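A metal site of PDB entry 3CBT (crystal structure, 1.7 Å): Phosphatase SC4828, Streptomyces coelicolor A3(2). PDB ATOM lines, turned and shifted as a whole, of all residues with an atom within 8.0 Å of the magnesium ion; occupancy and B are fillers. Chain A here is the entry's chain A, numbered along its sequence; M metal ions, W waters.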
ATOM      1  N   TYR A  36      -4.047  -3.549  -6.605  1.00  0.00           N
ATOM      2  CA  TYR A  36      -3.055  -4.085  -5.645  1.00  0.00           C
ATOM      3  C   TYR A  36      -3.061  -3.296  -4.356  1.00  0.00           C
ATOM      4  O   TYR A  36      -3.116  -2.082  -4.383  1.00  0.00           O
ATOM      5  CB  TYR A  36      -1.619  -4.084  -6.232  1.00  0.00           C
ATOM      6  CG  TYR A  36      -1.540  -5.020  -7.417  1.00  0.00           C
ATOM      7  CD1 TYR A  36      -1.237  -6.374  -7.230  1.00  0.00           C
ATOM      8  CD2 TYR A  36      -1.794  -4.547  -8.712  1.00  0.00           C
ATOM      9  CE1 TYR A  36      -1.225  -7.280  -8.339  1.00  0.00           C
ATOM     10  CE2 TYR A  36      -1.748  -5.415  -9.815  1.00  0.00           C
ATOM     11  CZ  TYR A  36      -1.427  -6.767  -9.623  1.00  0.00           C
ATOM     12  OH  TYR A  36      -1.455  -7.668 -10.678  1.00  0.00           O
ATOM     13  N   SER A 117      -0.550 -13.780 -12.593  1.00  0.00           N
ATOM     14  CA  SER A 117      -1.316 -13.432 -13.800  1.00  0.00           C
ATOM     15  C   SER A 117      -0.343 -13.309 -14.959  1.00  0.00           C
ATOM     16  O   SER A 117       0.869 -13.139 -14.730  1.00  0.00           O
ATOM     17  CB  SER A 117      -2.161 -12.152 -13.640  1.00  0.00           C
ATOM     18  OG  SER A 117      -1.427 -11.080 -13.107  1.00  0.00           O
ATOM     19  N   TRP A 119       0.436 -11.200 -18.480  1.00  0.00           N
ATOM     20  CA  TRP A 119       0.034  -9.972 -19.179  1.00  0.00           C
ATOM     21  C   TRP A 119       0.679  -9.945 -20.568  1.00  0.00           C
ATOM     22  O   TRP A 119       1.886 -10.264 -20.711  1.00  0.00           O
ATOM     23  CB  TRP A 119       0.479  -8.735 -18.422  1.00  0.00           C
ATOM     24  CG  TRP A 119       0.067  -8.627 -16.984  1.00  0.00           C
ATOM     25  CD1 TRP A 119      -0.744  -9.455 -16.276  1.00  0.00           C
ATOM     26  CD2 TRP A 119       0.439  -7.563 -16.110  1.00  0.00           C
ATOM     27  NE1 TRP A 119      -0.850  -9.010 -14.968  1.00  0.00           N
ATOM     28  CE2 TRP A 119      -0.135  -7.843 -14.845  1.00  0.00           C
ATOM     29  CE3 TRP A 119       1.221  -6.421 -16.268  1.00  0.00           C
ATOM     30  CZ2 TRP A 119       0.034  -6.997 -13.725  1.00  0.00           C
ATOM     31  CZ3 TRP A 119       1.410  -5.583 -15.171  1.00  0.00           C
ATOM     32  CH2 TRP A 119       0.810  -5.874 -13.898  1.00  0.00           C
ATOM     33  N   VAL A 133       4.855 -12.765 -16.821  1.00  0.00           N
ATOM     34  CA  VAL A 133       4.214 -13.462 -15.714  1.00  0.00           C
ATOM     35  C   VAL A 133       4.442 -12.633 -14.466  1.00  0.00           C
ATOM     36  O   VAL A 133       5.587 -12.395 -14.070  1.00  0.00           O
ATOM     37  CB  VAL A 133       4.852 -14.842 -15.521  1.00  0.00           C
ATOM     38  CG1 VAL A 133       4.194 -15.514 -14.317  1.00  0.00           C
ATOM     39  CG2 VAL A 133       4.806 -15.670 -16.843  1.00  0.00           C
ATOM     40  N   ASN A 134       3.349 -12.111 -13.887  1.00  0.00           N
ATOM     41  CA  ASN A 134       3.456 -11.306 -12.693  1.00  0.00           C
ATOM     42  C   ASN A 134       3.142 -12.201 -11.481  1.00  0.00           C
ATOM     43  O   ASN A 134       1.977 -12.575 -11.256  1.00  0.00           O
ATOM     44  CB  ASN A 134       2.466 -10.150 -12.733  1.00  0.00           C
ATOM     45  CG  ASN A 134       2.769  -9.130 -11.691  1.00  0.00           C
ATOM     46  OD1 ASN A 134       3.765  -8.439 -11.816  1.00  0.00           O
ATOM     47  ND2 ASN A 134       1.964  -9.051 -10.640  1.00  0.00           N
ATOM     48  N   LEU A 135       4.169 -12.616 -10.741  1.00  0.00           N
ATOM     49  CA  LEU A 135       3.914 -13.396  -9.521  1.00  0.00           C
ATOM     50  C   LEU A 135       3.217 -12.505  -8.460  1.00  0.00           C
ATOM     51  O   LEU A 135       3.643 -11.367  -8.209  1.00  0.00           O
ATOM     52  CB  LEU A 135       5.219 -13.972  -8.986  1.00  0.00           C
ATOM     53  CG  LEU A 135       5.943 -14.892 -10.000  1.00  0.00           C
ATOM     54  CD1 LEU A 135       7.266 -15.302  -9.398  1.00  0.00           C
ATOM     55  CD2 LEU A 135       5.130 -16.154 -10.291  1.00  0.00           C
ATOM     56  N   GLU A 136       2.171 -13.036  -7.845  1.00  0.00           N
ATOM     57  CA  GLU A 136       1.272 -12.181  -7.022  1.00  0.00           C
ATOM     58  C   GLU A 136       0.348 -13.069  -6.245  1.00  0.00           C
ATOM     59  O   GLU A 136       0.168 -14.260  -6.571  1.00  0.00           O
ATOM     60  CB  GLU A 136       0.457 -11.241  -7.962  1.00  0.00           C
ATOM     61  CG  GLU A 136      -0.684 -11.951  -8.728  1.00  0.00           C
ATOM     62  CD  GLU A 136      -1.249 -11.133  -9.928  1.00  0.00           C
ATOM     63  OE1 GLU A 136      -0.667 -10.131 -10.301  1.00  0.00           O
ATOM     64  OE2 GLU A 136      -2.269 -11.580 -10.496  1.00  0.00           O
ATOM     65  N   GLU A 149      -1.724  -8.651  -4.233  1.00  0.00           N
ATOM     66  CA  GLU A 149      -0.564  -8.056  -3.593  1.00  0.00           C
ATOM     67  C   GLU A 149       0.575  -8.535  -4.457  1.00  0.00           C
ATOM     68  O   GLU A 149       0.617  -9.703  -4.811  1.00  0.00           O
ATOM     69  CB  GLU A 149      -0.367  -8.578  -2.148  1.00  0.00           C
ATOM     70  CG  GLU A 149      -1.532  -8.373  -1.198  1.00  0.00           C
ATOM     71  CD  GLU A 149      -1.382  -9.251   0.052  1.00  0.00           C
ATOM     72  OE1 GLU A 149      -0.303  -9.878   0.241  1.00  0.00           O
ATOM     73  OE2 GLU A 149      -2.327  -9.330   0.855  1.00  0.00           O
ATOM     74  N   ASP A 150       1.479  -7.633  -4.829  1.00  0.00           N
ATOM     75  CA  ASP A 150       2.527  -8.037  -5.775  1.00  0.00           C
ATOM     76  C   ASP A 150       3.666  -8.790  -5.045  1.00  0.00           C
ATOM     77  O   ASP A 150       3.949  -8.513  -3.883  1.00  0.00           O
ATOM     78  CB  ASP A 150       2.983  -6.837  -6.600  1.00  0.00           C
ATOM     79  CG  ASP A 150       4.077  -7.192  -7.610  1.00  0.00           C
ATOM     80  OD1 ASP A 150       3.817  -7.488  -8.824  1.00  0.00           O
ATOM     81  OD2 ASP A 150       5.211  -7.111  -7.155  1.00  0.00           O
ATOM     82  N   HIS A 151       4.255  -9.777  -5.717  1.00  0.00           N
ATOM     83  CA  HIS A 151       5.260 -10.635  -5.083  1.00  0.00           C
ATOM     84  C   HIS A 151       6.658 -10.354  -5.679  1.00  0.00           C
ATOM     85  O   HIS A 151       7.571 -11.164  -5.516  1.00  0.00           O
ATOM     86  CB  HIS A 151       4.889 -12.104  -5.200  1.00  0.00           C
ATOM     87  CG  HIS A 151       3.760 -12.522  -4.315  1.00  0.00           C
ATOM     88  ND1 HIS A 151       3.068 -13.696  -4.497  1.00  0.00           N
ATOM     89  CD2 HIS A 151       3.176 -11.903  -3.255  1.00  0.00           C
ATOM     90  CE1 HIS A 151       2.128 -13.808  -3.581  1.00  0.00           C
ATOM     91  NE2 HIS A 151       2.159 -12.729  -2.817  1.00  0.00           N
ATOM     92  N   PHE A 152       6.775  -9.206  -6.338  1.00  0.00           N
ATOM     93  CA  PHE A 152       8.044  -8.578  -6.751  1.00  0.00           C
ATOM     94  C   PHE A 152       8.709  -9.215  -7.992  1.00  0.00           C
ATOM     95  O   PHE A 152       9.057  -8.533  -8.988  1.00  0.00           O
ATOM     96  CB  PHE A 152       9.003  -8.440  -5.538  1.00  0.00           C
ATOM     97  CG  PHE A 152       8.392  -7.678  -4.386  1.00  0.00           C
ATOM     98  CD1 PHE A 152       8.313  -6.294  -4.417  1.00  0.00           C
ATOM     99  CD2 PHE A 152       7.821  -8.353  -3.306  1.00  0.00           C
ATOM    100  CE1 PHE A 152       7.709  -5.586  -3.355  1.00  0.00           C
ATOM    101  CE2 PHE A 152       7.220  -7.657  -2.249  1.00  0.00           C
ATOM    102  CZ  PHE A 152       7.158  -6.281  -2.289  1.00  0.00           C
ATOM    103  N   LEU A 153       8.833 -10.522  -7.947  1.00  0.00           N
ATOM    104  CA  LEU A 153       9.501 -11.240  -9.020  1.00  0.00           C
ATOM    105  C   LEU A 153       8.586 -11.388 -10.256  1.00  0.00           C
ATOM    106  O   LEU A 153       7.409 -11.714 -10.148  1.00  0.00           O
ATOM    107  CB  LEU A 153       9.939 -12.587  -8.480  1.00  0.00           C
ATOM    108  CG  LEU A 153      10.709 -13.526  -9.407  1.00  0.00           C
ATOM    109  CD1 LEU A 153      12.086 -12.891  -9.754  1.00  0.00           C
ATOM    110  CD2 LEU A 153      10.840 -14.864  -8.673  1.00  0.00           C
ATOM    111  N   ASP A 154       9.143 -11.162 -11.427  1.00  0.00           N
ATOM    112  CA  ASP A 154       8.382 -11.334 -12.663  1.00  0.00           C
ATOM    113  C   ASP A 154       9.165 -12.256 -13.602  1.00  0.00           C
ATOM    114  O   ASP A 154      10.365 -12.530 -13.382  1.00  0.00           O
ATOM    115  CB  ASP A 154       8.199  -9.982 -13.368  1.00  0.00           C
ATOM    116  CG  ASP A 154       7.520  -8.918 -12.491  1.00  0.00           C
ATOM    117  OD1 ASP A 154       6.589  -9.246 -11.763  1.00  0.00           O
ATOM    118  OD2 ASP A 154       7.934  -7.741 -12.533  1.00  0.00           O
ATOM    119  N   ILE A 155       8.477 -12.738 -14.649  1.00  0.00           N
ATOM    120  CA  ILE A 155       9.113 -13.532 -15.696  1.00  0.00           C
ATOM    121  C   ILE A 155       8.715 -12.926 -17.019  1.00  0.00           C
ATOM    122  O   ILE A 155       7.539 -12.574 -17.237  1.00  0.00           O
ATOM    123  CB  ILE A 155       8.658 -15.034 -15.680  1.00  0.00           C
ATOM    124  CG1 ILE A 155       8.836 -15.657 -14.270  1.00  0.00           C
ATOM    125  CG2 ILE A 155       9.439 -15.816 -16.666  1.00  0.00           C
ATOM    126  CD1 ILE A 155       8.237 -17.051 -14.117  1.00  0.00           C
ATOM    127  N   ARG A 166      12.622 -11.191 -14.314  1.00  0.00           N
ATOM    128  CA  ARG A 166      12.730  -9.727 -14.270  1.00  0.00           C
ATOM    129  C   ARG A 166      12.527  -9.310 -12.833  1.00  0.00           C
ATOM    130  O   ARG A 166      11.811  -9.965 -12.080  1.00  0.00           O
ATOM    131  CB  ARG A 166      11.687  -9.091 -15.163  1.00  0.00           C
ATOM    132  CG  ARG A 166      11.997  -9.178 -16.637  1.00  0.00           C
ATOM    133  CD  ARG A 166      12.954  -8.084 -17.066  1.00  0.00           C
ATOM    134  NE  ARG A 166      12.641  -7.566 -18.411  1.00  0.00           N
ATOM    135  CZ  ARG A 166      13.563  -7.133 -19.274  1.00  0.00           C
ATOM    136  NH1 ARG A 166      14.846  -7.186 -18.966  1.00  0.00           N
ATOM    137  NH2 ARG A 166      13.188  -6.672 -20.470  1.00  0.00           N
ATOM    138  N   ASP A 167      13.157  -8.208 -12.449  1.00  0.00           N
ATOM    139  CA  ASP A 167      13.046  -7.652 -11.092  1.00  0.00           C
ATOM    140  C   ASP A 167      13.519  -8.555  -9.934  1.00  0.00           C
ATOM    141  O   ASP A 167      13.041  -8.436  -8.795  1.00  0.00           O
ATOM    142  CB  ASP A 167      11.627  -7.119 -10.839  1.00  0.00           C
ATOM    143  CG  ASP A 167      11.241  -5.962 -11.763  1.00  0.00           C
ATOM    144  OD1 ASP A 167      12.111  -5.309 -12.347  1.00  0.00           O
ATOM    145  OD2 ASP A 167      10.017  -5.717 -11.877  1.00  0.00           O
ATOM    146  N   GLU A 170      14.714  -6.356  -7.087  1.00  0.00           N
ATOM    147  CA  GLU A 170      13.608  -5.858  -6.245  1.00  0.00           C
ATOM    148  C   GLU A 170      13.115  -6.947  -5.297  1.00  0.00           C
ATOM    149  O   GLU A 170      12.890  -6.691  -4.120  1.00  0.00           O
ATOM    150  CB  GLU A 170      12.463  -5.318  -7.108  1.00  0.00           C
ATOM    151  CG  GLU A 170      12.922  -4.129  -7.962  1.00  0.00           C
ATOM    152  CD  GLU A 170      11.809  -3.359  -8.641  1.00  0.00           C
ATOM    153  OE1 GLU A 170      10.777  -3.962  -8.988  1.00  0.00           O
ATOM    154  OE2 GLU A 170      11.976  -2.132  -8.872  1.00  0.00           O
HETATM  155 MG    MG M   1       5.332  -8.007 -10.419  1.00  0.00          MG
HETATM  156  O   HOH W   1       5.395  -9.830  -9.369  1.00  0.00           O
HETATM  157  O   HOH W   2       6.818  -7.142  -9.134  1.00  0.00           O
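Of the 17 residues printed, 3 come within 4 Å of the magnesium ion.
Water W1 lies within hydrogen-bond range of O of Leu 135, O of Leu 153 and N of Phe 152. Water W2 bridges OD2 of Asp 150 and O of Phe 152.
The magnesium ion is bound by water W1 (2.1 Å), the side-chain amide oxygen (OD1) of Asn 134 (2.1 Å), water W2 (2.1 Å), the side-chain carboxylate (OD1) of Asp 154 (2.2 Å) and the side-chain carboxylate (OD1) of Asp 150 (2.3 Å). The magnesium ion has five donor atoms within binding distance.
The side-chain amide nitrogen of Asn 134 sits at hydrogen-bond distance from the side-chain carboxylate of Glu 136. N of Asn 134 sits at hydrogen-bond distance from O of Ser 117 (2.8 Å). The backbone carbonyl oxygen (O) of Asp 154 sits at hydrogen-bond distance from the backbone NH (N) of Arg 166 (2.8 Å). The backbone NH (N) of Phe 152 is in hydrogen-bond range of the side-chain carboxylate (OD2) of Asp 150, at 2.7 Å.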
